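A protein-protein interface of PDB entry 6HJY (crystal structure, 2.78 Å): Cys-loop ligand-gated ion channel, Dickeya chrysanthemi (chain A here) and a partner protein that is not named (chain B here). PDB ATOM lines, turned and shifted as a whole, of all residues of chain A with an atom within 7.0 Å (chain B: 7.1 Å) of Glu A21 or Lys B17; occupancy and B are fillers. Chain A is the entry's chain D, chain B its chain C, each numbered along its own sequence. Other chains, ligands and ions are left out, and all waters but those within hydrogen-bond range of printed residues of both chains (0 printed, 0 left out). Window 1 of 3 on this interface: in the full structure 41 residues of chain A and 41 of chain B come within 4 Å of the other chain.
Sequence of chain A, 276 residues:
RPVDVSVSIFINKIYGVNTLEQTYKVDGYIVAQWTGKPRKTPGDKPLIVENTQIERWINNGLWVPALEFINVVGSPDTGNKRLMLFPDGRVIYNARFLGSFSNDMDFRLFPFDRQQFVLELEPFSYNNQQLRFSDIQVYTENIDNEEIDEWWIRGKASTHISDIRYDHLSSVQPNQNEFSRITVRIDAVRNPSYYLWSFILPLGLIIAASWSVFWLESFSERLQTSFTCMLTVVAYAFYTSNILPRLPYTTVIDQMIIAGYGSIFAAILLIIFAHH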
ATOM      1  N   ASN A  18      14.491  19.519  16.137  1.00  0.00           N
ATOM      2  CA  ASN A  18      15.215  18.758  17.143  1.00  0.00           C
ATOM      3  C   ASN A  18      16.683  18.930  16.775  1.00  0.00           C
ATOM      4  O   ASN A  18      17.163  18.315  15.817  1.00  0.00           O
ATOM      5  CB  ASN A  18      14.798  17.288  17.137  1.00  0.00           C
ATOM      6  CG  ASN A  18      15.435  16.453  18.226  1.00  0.00           C
ATOM      7  OD1 ASN A  18      16.635  16.545  18.510  1.00  0.00           O
ATOM      8  ND2 ASN A  18      14.650  15.570  18.819  1.00  0.00           N
ATOM      9  N   THR A  19      17.366  19.823  17.511  1.00  0.00           N
ATOM     10  CA  THR A  19      18.769  20.204  17.330  1.00  0.00           C
ATOM     11  C   THR A  19      19.740  19.035  17.380  1.00  0.00           C
ATOM     12  O   THR A  19      20.634  18.951  16.534  1.00  0.00           O
ATOM     13  CB  THR A  19      19.184  21.252  18.360  1.00  0.00           C
ATOM     14  OG1 THR A  19      18.893  20.751  19.664  1.00  0.00           O
ATOM     15  CG2 THR A  19      18.519  22.603  18.132  1.00  0.00           C
ATOM     16  N   LEU A  20      19.584  18.149  18.382  1.00  0.00           N
ATOM     17  CA  LEU A  20      20.483  17.011  18.549  1.00  0.00           C
ATOM     18  C   LEU A  20      20.305  15.960  17.470  1.00  0.00           C
ATOM     19  O   LEU A  20      21.301  15.432  16.979  1.00  0.00           O
ATOM     20  CB  LEU A  20      20.384  16.403  19.958  1.00  0.00           C
ATOM     21  CG  LEU A  20      21.590  15.573  20.449  1.00  0.00           C
ATOM     22  CD1 LEU A  20      22.932  16.291  20.196  1.00  0.00           C
ATOM     23  CD2 LEU A  20      21.449  15.244  21.925  1.00  0.00           C
ATOM     24  N   GLU A  21      19.053  15.679  17.072  1.00  0.00           N
ATOM     25  CA  GLU A  21      18.760  14.696  16.027  1.00  0.00           C
ATOM     26  C   GLU A  21      18.934  15.249  14.604  1.00  0.00           C
ATOM     27  O   GLU A  21      18.981  14.458  13.654  1.00  0.00           O
ATOM     28  CB  GLU A  21      17.342  14.134  16.193  1.00  0.00           C
ATOM     29  CG  GLU A  21      17.216  13.093  17.290  1.00  0.00           C
ATOM     30  CD  GLU A  21      15.869  12.395  17.399  1.00  0.00           C
ATOM     31  OE1 GLU A  21      14.935  12.749  16.639  1.00  0.00           O
ATOM     32  OE2 GLU A  21      15.747  11.486  18.252  1.00  0.00           O
ATOM     33  N   GLN A  22      19.011  16.601  14.465  1.00  0.00           N
ATOM     34  CA  GLN A  22      19.089  17.341  13.197  1.00  0.00           C
ATOM     35  C   GLN A  22      17.865  17.032  12.314  1.00  0.00           C
ATOM     36  O   GLN A  22      18.001  16.684  11.140  1.00  0.00           O
ATOM     37  CB  GLN A  22      20.430  17.126  12.470  1.00  0.00           C
ATOM     38  CG  GLN A  22      21.558  18.008  12.998  1.00  0.00           C
ATOM     39  CD  GLN A  22      22.872  17.675  12.341  1.00  0.00           C
ATOM     40  OE1 GLN A  22      23.248  18.247  11.321  1.00  0.00           O
ATOM     41  NE2 GLN A  22      23.594  16.719  12.899  1.00  0.00           N
ATOM     42  N   THR A  23      16.664  17.151  12.911  1.00  0.00           N
ATOM     43  CA  THR A  23      15.369  16.890  12.277  1.00  0.00           C
ATOM     44  C   THR A  23      14.390  18.047  12.513  1.00  0.00           C
ATOM     45  O   THR A  23      14.597  18.869  13.405  1.00  0.00           O
ATOM     46  CB  THR A  23      14.768  15.558  12.769  1.00  0.00           C
ATOM     47  OG1 THR A  23      14.572  15.614  14.182  1.00  0.00           O
ATOM     48  CG2 THR A  23      15.604  14.342  12.384  1.00  0.00           C
ATOM     49  N   TYR A  24      13.317  18.090  11.710  1.00  0.00           N
ATOM     50  CA  TYR A  24      12.249  19.093  11.728  1.00  0.00           C
ATOM     51  C   TYR A  24      10.974  18.475  11.155  1.00  0.00           C
ATOM     52  O   TYR A  24      11.039  17.586  10.307  1.00  0.00           O
ATOM     53  CB  TYR A  24      12.655  20.364  10.936  1.00  0.00           C
ATOM     54  CG  TYR A  24      13.257  20.078   9.572  1.00  0.00           C
ATOM     55  CD1 TYR A  24      14.620  19.827   9.431  1.00  0.00           C
ATOM     56  CD2 TYR A  24      12.473  20.085   8.423  1.00  0.00           C
ATOM     57  CE1 TYR A  24      15.176  19.529   8.190  1.00  0.00           C
ATOM     58  CE2 TYR A  24      13.024  19.812   7.169  1.00  0.00           C
ATOM     59  CZ  TYR A  24      14.377  19.528   7.061  1.00  0.00           C
ATOM     60  OH  TYR A  24      14.949  19.251   5.849  1.00  0.00           O
ATOM     61  N   VAL A  73      12.340  10.720   8.189  1.00  0.00           N
ATOM     62  CA  VAL A  73      12.773   9.918   9.332  1.00  0.00           C
ATOM     63  C   VAL A  73      11.545   9.128   9.789  1.00  0.00           C
ATOM     64  O   VAL A  73      10.646   9.678  10.434  1.00  0.00           O
ATOM     65  CB  VAL A  73      13.393  10.787  10.453  1.00  0.00           C
ATOM     66  CG1 VAL A  73      14.072   9.913  11.489  1.00  0.00           C
ATOM     67  CG2 VAL A  73      14.393  11.786   9.885  1.00  0.00           C
ATOM     68  N   SER A 100       8.736  13.773   9.708  1.00  0.00           N
ATOM     69  CA  SER A 100       9.931  14.280  10.363  1.00  0.00           C
ATOM     70  C   SER A 100      11.018  14.159   9.307  1.00  0.00           C
ATOM     71  O   SER A 100      11.206  13.081   8.747  1.00  0.00           O
ATOM     72  CB  SER A 100      10.265  13.452  11.600  1.00  0.00           C
ATOM     73  OG  SER A 100       9.582  13.945  12.740  1.00  0.00           O
ATOM     74  N   PHE A 101      11.649  15.286   8.956  1.00  0.00           N
ATOM     75  CA  PHE A 101      12.680  15.345   7.929  1.00  0.00           C
ATOM     76  C   PHE A 101      14.012  15.740   8.515  1.00  0.00           C
ATOM     77  O   PHE A 101      14.076  16.609   9.376  1.00  0.00           O
ATOM     78  CB  PHE A 101      12.276  16.295   6.782  1.00  0.00           C
ATOM     79  CG  PHE A 101      11.057  15.857   5.998  1.00  0.00           C
ATOM     80  CD1 PHE A 101       9.777  16.182   6.435  1.00  0.00           C
ATOM     81  CD2 PHE A 101      11.190  15.146   4.811  1.00  0.00           C
ATOM     82  CE1 PHE A 101       8.649  15.769   5.719  1.00  0.00           C
ATOM     83  CE2 PHE A 101      10.061  14.739   4.089  1.00  0.00           C
ATOM     84  CZ  PHE A 101       8.799  15.047   4.555  1.00  0.00           C
ATOM     85  N   SER A 102      15.072  15.085   8.047  1.00  0.00           N
ATOM     86  CA  SER A 102      16.441  15.329   8.472  1.00  0.00           C
ATOM     87  C   SER A 102      17.201  16.106   7.412  1.00  0.00           C
ATOM     88  O   SER A 102      16.874  16.028   6.230  1.00  0.00           O
ATOM     89  CB  SER A 102      17.155  14.012   8.754  1.00  0.00           C
ATOM     90  OG  SER A 102      17.194  13.188   7.598  1.00  0.00           O
ATOM     91  N   ASN A 103      18.208  16.866   7.854  1.00  0.00           N
ATOM     92  CA  ASN A 103      19.120  17.666   7.037  1.00  0.00           C
ATOM     93  C   ASN A 103      20.273  18.144   7.923  1.00  0.00           C
ATOM     94  O   ASN A 103      20.143  18.114   9.153  1.00  0.00           O
ATOM     95  CB  ASN A 103      18.401  18.870   6.394  1.00  0.00           C
ATOM     96  CG  ASN A 103      19.160  19.533   5.264  1.00  0.00           C
ATOM     97  OD1 ASN A 103      19.976  18.923   4.559  1.00  0.00           O
ATOM     98  ND2 ASN A 103      18.895  20.806   5.059  1.00  0.00           N
ATOM     99  N   MET A 105      22.221  20.435   9.969  1.00  0.00           N
ATOM    100  CA  MET A 105      21.851  21.627  10.712  1.00  0.00           C
ATOM    101  C   MET A 105      22.972  22.063  11.630  1.00  0.00           C
ATOM    102  O   MET A 105      23.333  21.336  12.561  1.00  0.00           O
ATOM    103  CB  MET A 105      20.537  21.408  11.488  1.00  0.00           C
ATOM    104  CG  MET A 105      19.345  21.006  10.627  1.00  0.00           C
ATOM    105  SD  MET A 105      17.787  21.628  11.272  1.00  0.00           S
ATOM    106  CE  MET A 105      17.438  20.443  12.465  1.00  0.00           C
ATOM    107  N   PHE A 107      24.084  24.609  14.331  1.00  0.00           N
ATOM    108  CA  PHE A 107      23.580  25.516  15.354  1.00  0.00           C
ATOM    109  C   PHE A 107      24.688  26.253  16.116  1.00  0.00           C
ATOM    110  O   PHE A 107      24.403  26.832  17.162  1.00  0.00           O
ATOM    111  CB  PHE A 107      22.667  24.763  16.331  1.00  0.00           C
ATOM    112  CG  PHE A 107      21.518  24.027  15.694  1.00  0.00           C
ATOM    113  CD1 PHE A 107      20.329  24.681  15.400  1.00  0.00           C
ATOM    114  CD2 PHE A 107      21.610  22.671  15.422  1.00  0.00           C
ATOM    115  CE1 PHE A 107      19.261  23.993  14.823  1.00  0.00           C
ATOM    116  CE2 PHE A 107      20.541  21.982  14.859  1.00  0.00           C
ATOM    117  CZ  PHE A 107      19.371  22.645  14.566  1.00  0.00           C
ATOM    118  N   ARG A 246      19.899  20.880  23.297  1.00  0.00           N
ATOM    119  CA  ARG A 246      21.012  19.952  23.472  1.00  0.00           C
ATOM    120  C   ARG A 246      21.851  19.829  22.211  1.00  0.00           C
ATOM    121  O   ARG A 246      21.322  19.522  21.139  1.00  0.00           O
ATOM    122  CB  ARG A 246      20.554  18.591  24.028  1.00  0.00           C
ATOM    123  CG  ARG A 246      20.165  18.668  25.512  1.00  0.00           C
ATOM    124  CD  ARG A 246      21.358  18.714  26.484  1.00  0.00           C
ATOM    125  NE  ARG A 246      22.311  19.799  26.193  1.00  0.00           N
ATOM    126  CZ  ARG A 246      22.222  21.045  26.658  1.00  0.00           C
ATOM    127  NH1 ARG A 246      21.227  21.394  27.465  1.00  0.00           N
ATOM    128  NH2 ARG A 246      23.126  21.953  26.310  1.00  0.00           N
ATOM    129  N   PHE B  14      22.433  -0.350   3.659  1.00  0.00           N
ATOM    130  CA  PHE B  14      22.793   1.050   3.447  1.00  0.00           C
ATOM    131  C   PHE B  14      22.463   1.785   4.729  1.00  0.00           C
ATOM    132  O   PHE B  14      21.308   1.783   5.146  1.00  0.00           O
ATOM    133  CB  PHE B  14      22.029   1.634   2.245  1.00  0.00           C
ATOM    134  CG  PHE B  14      22.404   1.006   0.919  1.00  0.00           C
ATOM    135  CD1 PHE B  14      21.855  -0.212   0.524  1.00  0.00           C
ATOM    136  CD2 PHE B  14      23.280   1.649   0.050  1.00  0.00           C
ATOM    137  CE1 PHE B  14      22.206  -0.796  -0.698  1.00  0.00           C
ATOM    138  CE2 PHE B  14      23.620   1.070  -1.183  1.00  0.00           C
ATOM    139  CZ  PHE B  14      23.087  -0.152  -1.543  1.00  0.00           C
ATOM    140  N   ILE B  15      23.478   2.333   5.405  1.00  0.00           N
ATOM    141  CA  ILE B  15      23.245   3.029   6.665  1.00  0.00           C
ATOM    142  C   ILE B  15      23.241   4.527   6.408  1.00  0.00           C
ATOM    143  O   ILE B  15      24.283   5.116   6.108  1.00  0.00           O
ATOM    144  CB  ILE B  15      24.201   2.551   7.793  1.00  0.00           C
ATOM    145  CG1 ILE B  15      23.915   1.066   8.154  1.00  0.00           C
ATOM    146  CG2 ILE B  15      24.082   3.454   9.031  1.00  0.00           C
ATOM    147  CD1 ILE B  15      25.108   0.280   8.669  1.00  0.00           C
ATOM    148  N   ASN B  16      22.047   5.124   6.473  1.00  0.00           N
ATOM    149  CA  ASN B  16      21.859   6.550   6.236  1.00  0.00           C
ATOM    150  C   ASN B  16      22.202   7.362   7.472  1.00  0.00           C
ATOM    151  O   ASN B  16      22.813   8.418   7.353  1.00  0.00           O
ATOM    152  CB  ASN B  16      20.410   6.858   5.796  1.00  0.00           C
ATOM    153  CG  ASN B  16      19.942   6.166   4.529  1.00  0.00           C
ATOM    154  OD1 ASN B  16      20.687   5.991   3.551  1.00  0.00           O
ATOM    155  ND2 ASN B  16      18.664   5.806   4.510  1.00  0.00           N
ATOM    156  N   LYS B  17      21.807   6.868   8.653  1.00  0.00           N
ATOM    157  CA  LYS B  17      21.951   7.571   9.917  1.00  0.00           C
ATOM    158  C   LYS B  17      22.017   6.593  11.094  1.00  0.00           C
ATOM    159  O   LYS B  17      21.350   5.557  11.086  1.00  0.00           O
ATOM    160  CB  LYS B  17      20.690   8.444  10.093  1.00  0.00           C
ATOM    161  CG  LYS B  17      20.877   9.829  10.703  1.00  0.00           C
ATOM    162  CD  LYS B  17      19.510  10.546  10.756  1.00  0.00           C
ATOM    163  CE  LYS B  17      19.397  11.609  11.825  1.00  0.00           C
ATOM    164  NZ  LYS B  17      19.757  12.957  11.311  1.00  0.00           N
ATOM    165  N   ILE B  18      22.841   6.934  12.093  1.00  0.00           N
ATOM    166  CA  ILE B  18      22.964   6.291  13.402  1.00  0.00           C
ATOM    167  C   ILE B  18      22.840   7.487  14.338  1.00  0.00           C
ATOM    168  O   ILE B  18      23.643   8.425  14.250  1.00  0.00           O
ATOM    169  CB  ILE B  18      24.254   5.464  13.649  1.00  0.00           C
ATOM    170  CG1 ILE B  18      24.426   4.358  12.576  1.00  0.00           C
ATOM    171  CG2 ILE B  18      24.223   4.873  15.080  1.00  0.00           C
ATOM    172  CD1 ILE B  18      25.731   3.530  12.650  1.00  0.00           C
ATOM    173  N   TYR B  19      21.786   7.503  15.156  1.00  0.00           N
ATOM    174  CA  TYR B  19      21.471   8.629  16.032  1.00  0.00           C
ATOM    175  C   TYR B  19      20.587   8.174  17.206  1.00  0.00           C
ATOM    176  O   TYR B  19      20.337   6.980  17.362  1.00  0.00           O
ATOM    177  CB  TYR B  19      20.764   9.738  15.195  1.00  0.00           C
ATOM    178  CG  TYR B  19      19.345   9.385  14.788  1.00  0.00           C
ATOM    179  CD1 TYR B  19      19.098   8.478  13.756  1.00  0.00           C
ATOM    180  CD2 TYR B  19      18.251   9.946  15.434  1.00  0.00           C
ATOM    181  CE1 TYR B  19      17.795   8.126  13.402  1.00  0.00           C
ATOM    182  CE2 TYR B  19      16.946   9.600  15.090  1.00  0.00           C
ATOM    183  CZ  TYR B  19      16.725   8.689  14.073  1.00  0.00           C
ATOM    184  OH  TYR B  19      15.438   8.344  13.763  1.00  0.00           O
ATOM    185  N   GLY B  20      20.135   9.137  18.005  1.00  0.00           N
ATOM    186  CA  GLY B  20      19.232   8.924  19.134  1.00  0.00           C
ATOM    187  C   GLY B  20      19.649   7.855  20.121  1.00  0.00           C
ATOM    188  O   GLY B  20      18.823   7.019  20.498  1.00  0.00           O
ATOM    189  N   VAL B  21      20.939   7.875  20.537  1.00  0.00           N
ATOM    190  CA  VAL B  21      21.493   6.934  21.522  1.00  0.00           C
ATOM    191  C   VAL B  21      20.800   7.168  22.876  1.00  0.00           C
ATOM    192  O   VAL B  21      20.660   8.312  23.314  1.00  0.00           O
ATOM    193  CB  VAL B  21      23.052   6.988  21.632  1.00  0.00           C
ATOM    194  CG1 VAL B  21      23.574   6.087  22.753  1.00  0.00           C
ATOM    195  CG2 VAL B  21      23.716   6.606  20.313  1.00  0.00           C
ATOM    196  N   LYS B  29      19.177   4.511  17.258  1.00  0.00           N
ATOM    197  CA  LYS B  29      18.294   4.480  16.098  1.00  0.00           C
ATOM    198  C   LYS B  29      19.095   4.383  14.818  1.00  0.00           C
ATOM    199  O   LYS B  29      20.091   5.082  14.663  1.00  0.00           O
ATOM    200  CB  LYS B  29      17.388   5.715  16.087  1.00  0.00           C
ATOM    201  CG  LYS B  29      16.251   5.635  17.095  1.00  0.00           C
ATOM    202  CD  LYS B  29      15.711   7.018  17.346  1.00  0.00           C
ATOM    203  CE  LYS B  29      14.476   6.991  18.208  1.00  0.00           C
ATOM    204  NZ  LYS B  29      14.185   8.335  18.778  1.00  0.00           N
ATOM    205  N   VAL B  30      18.677   3.494  13.908  1.00  0.00           N
ATOM    206  CA  VAL B  30      19.340   3.317  12.614  1.00  0.00           C
ATOM    207  C   VAL B  30      18.307   3.518  11.488  1.00  0.00           C
ATOM    208  O   VAL B  30      17.239   2.900  11.511  1.00  0.00           O
ATOM    209  CB  VAL B  30      20.112   1.960  12.474  1.00  0.00           C
ATOM    210  CG1 VAL B  30      20.823   1.864  11.122  1.00  0.00           C
ATOM    211  CG2 VAL B  30      21.124   1.765  13.606  1.00  0.00           C
ATOM    212  N   ASP B  31      18.620   4.405  10.526  1.00  0.00           N
ATOM    213  CA  ASP B  31      17.806   4.619   9.331  1.00  0.00           C
ATOM    214  C   ASP B  31      18.636   4.108   8.165  1.00  0.00           C
ATOM    215  O   ASP B  31      19.835   4.399   8.097  1.00  0.00           O
ATOM    216  CB  ASP B  31      17.430   6.104   9.127  1.00  0.00           C
ATOM    217  CG  ASP B  31      16.635   6.374   7.847  1.00  0.00           C
ATOM    218  OD1 ASP B  31      15.434   6.030   7.809  1.00  0.00           O
ATOM    219  OD2 ASP B  31      17.214   6.936   6.894  1.00  0.00           O
ATOM    220  N   GLY B  32      18.014   3.322   7.295  1.00  0.00           N
ATOM    221  CA  GLY B  32      18.711   2.783   6.136  1.00  0.00           C
ATOM    222  C   GLY B  32      17.866   1.957   5.194  1.00  0.00           C
ATOM    223  O   GLY B  32      16.635   2.002   5.234  1.00  0.00           O
ATOM    224  N   LEU B 102      13.647   2.039   9.602  1.00  0.00           N
ATOM    225  CA  LEU B 102      14.028   2.872  10.738  1.00  0.00           C
ATOM    226  C   LEU B 102      13.726   2.049  11.972  1.00  0.00           C
ATOM    227  O   LEU B 102      12.580   1.651  12.166  1.00  0.00           O
ATOM    228  CB  LEU B 102      13.297   4.225  10.789  1.00  0.00           C
ATOM    229  CG  LEU B 102      13.587   5.056  12.053  1.00  0.00           C
ATOM    230  CD1 LEU B 102      15.019   5.592  12.068  1.00  0.00           C
ATOM    231  CD2 LEU B 102      12.593   6.162  12.231  1.00  0.00           C
ATOM    232  N   GLU B 145      27.155   6.528   4.808  1.00  0.00           N
ATOM    233  CA  GLU B 145      27.077   7.929   4.388  1.00  0.00           C
ATOM    234  C   GLU B 145      28.447   8.604   4.208  1.00  0.00           C
ATOM    235  O   GLU B 145      29.382   8.335   4.969  1.00  0.00           O
ATOM    236  CB  GLU B 145      26.249   8.706   5.421  1.00  0.00           C
ATOM    237  CG  GLU B 145      25.618   9.994   4.921  1.00  0.00           C
ATOM    238  CD  GLU B 145      24.591  10.594   5.871  1.00  0.00           C
ATOM    239  OE1 GLU B 145      24.963  10.952   7.014  1.00  0.00           O
ATOM    240  OE2 GLU B 145      23.405  10.693   5.481  1.00  0.00           O
ATOM    241  N   GLU B 154      27.529  14.477  16.562  1.00  0.00           N
ATOM    242  CA  GLU B 154      27.682  13.951  17.922  1.00  0.00           C
ATOM    243  C   GLU B 154      28.669  12.779  17.977  1.00  0.00           C
ATOM    244  O   GLU B 154      29.421  12.650  18.950  1.00  0.00           O
ATOM    245  CB  GLU B 154      26.312  13.532  18.490  1.00  0.00           C
ATOM    246  CG  GLU B 154      26.317  13.294  19.995  1.00  0.00           C
ATOM    247  CD  GLU B 154      25.002  12.876  20.637  1.00  0.00           C
ATOM    248  OE1 GLU B 154      23.966  12.832  19.934  1.00  0.00           O
ATOM    249  OE2 GLU B 154      25.008  12.607  21.860  1.00  0.00           O
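The side-chain amino group (NZ) of Lys B29 is in salt-bridge range of the side-chain carboxylate (OE2) of Glu A21 (3.6 Å). The backbone carbonyl oxygen of Glu A21 is in hydrogen-bond range of the side-chain amino group of Lys B17.
OD1 of Asn A18 sits at hydrogen-bond distance from N of Leu A20, 3.4 Å away. O of Lys B17 lies within hydrogen-bond range of N of Asp B31 (3.0 Å). N of Val A73 is in hydrogen-bond range of O of Ser A100. The side-chain amide oxygen (OD1) of Asn A18 lies within hydrogen-bond range of the backbone NH (N) of Glu A21 (2.9 Å). O of Tyr B19 lies within hydrogen-bond range of N of Lys B29, at 2.7 Å.
OE1 of Glu B154 touches CD1 of Leu A20 (3.6 Å). CD of Glu A21 touches CE2 of Tyr B19, 3.8 Å away. Tyr B19 touches Val A73 (OH to CG1, 3.1 Å). Val A73 touches Leu B102. NZ of Lys B17 touches CB of Ser A102 (3.8 Å).
Of chain B, only Lys B17, Tyr B19 and Lys B29 come within 4 Å of Glu A21. Lys B17 touches just these residues of chain A: Glu A21 (2.9 Å) and Ser A102 (3.8 Å). Of the printed residues of chain A, Glu B154 touches Leu A20. Printed residues of chain B within 4 Å of Ser A102: Lys B17 (3.8 Å). Printed residues of chain A within 4 Å of Tyr B19: Glu A21 (3.8 Å) and Val A73 (3.1 Å). Of the printed residues of chain A, Lys B29 touches Glu A21. Of the printed residues of chain B, Leu A20 touches Glu B154 (3.6 Å). Glu B145 touches none of the printed residues of chain A. Phe A101 touches none of the printed residues of chain B. The nearest residue of chain A that does not touch Lys B17 is Gln A22 (4.1 Å).
Hydrophobic or aromatic side chains of chain B within 4 Å of the printed part of chain A: Tyr B19 and Leu B102. Printed residues of chain A that touch a printed residue of chain B: Leu A20, Glu A21, Val A73 and Ser A102. Among the printed residues, 7 pairs touch across the chains.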
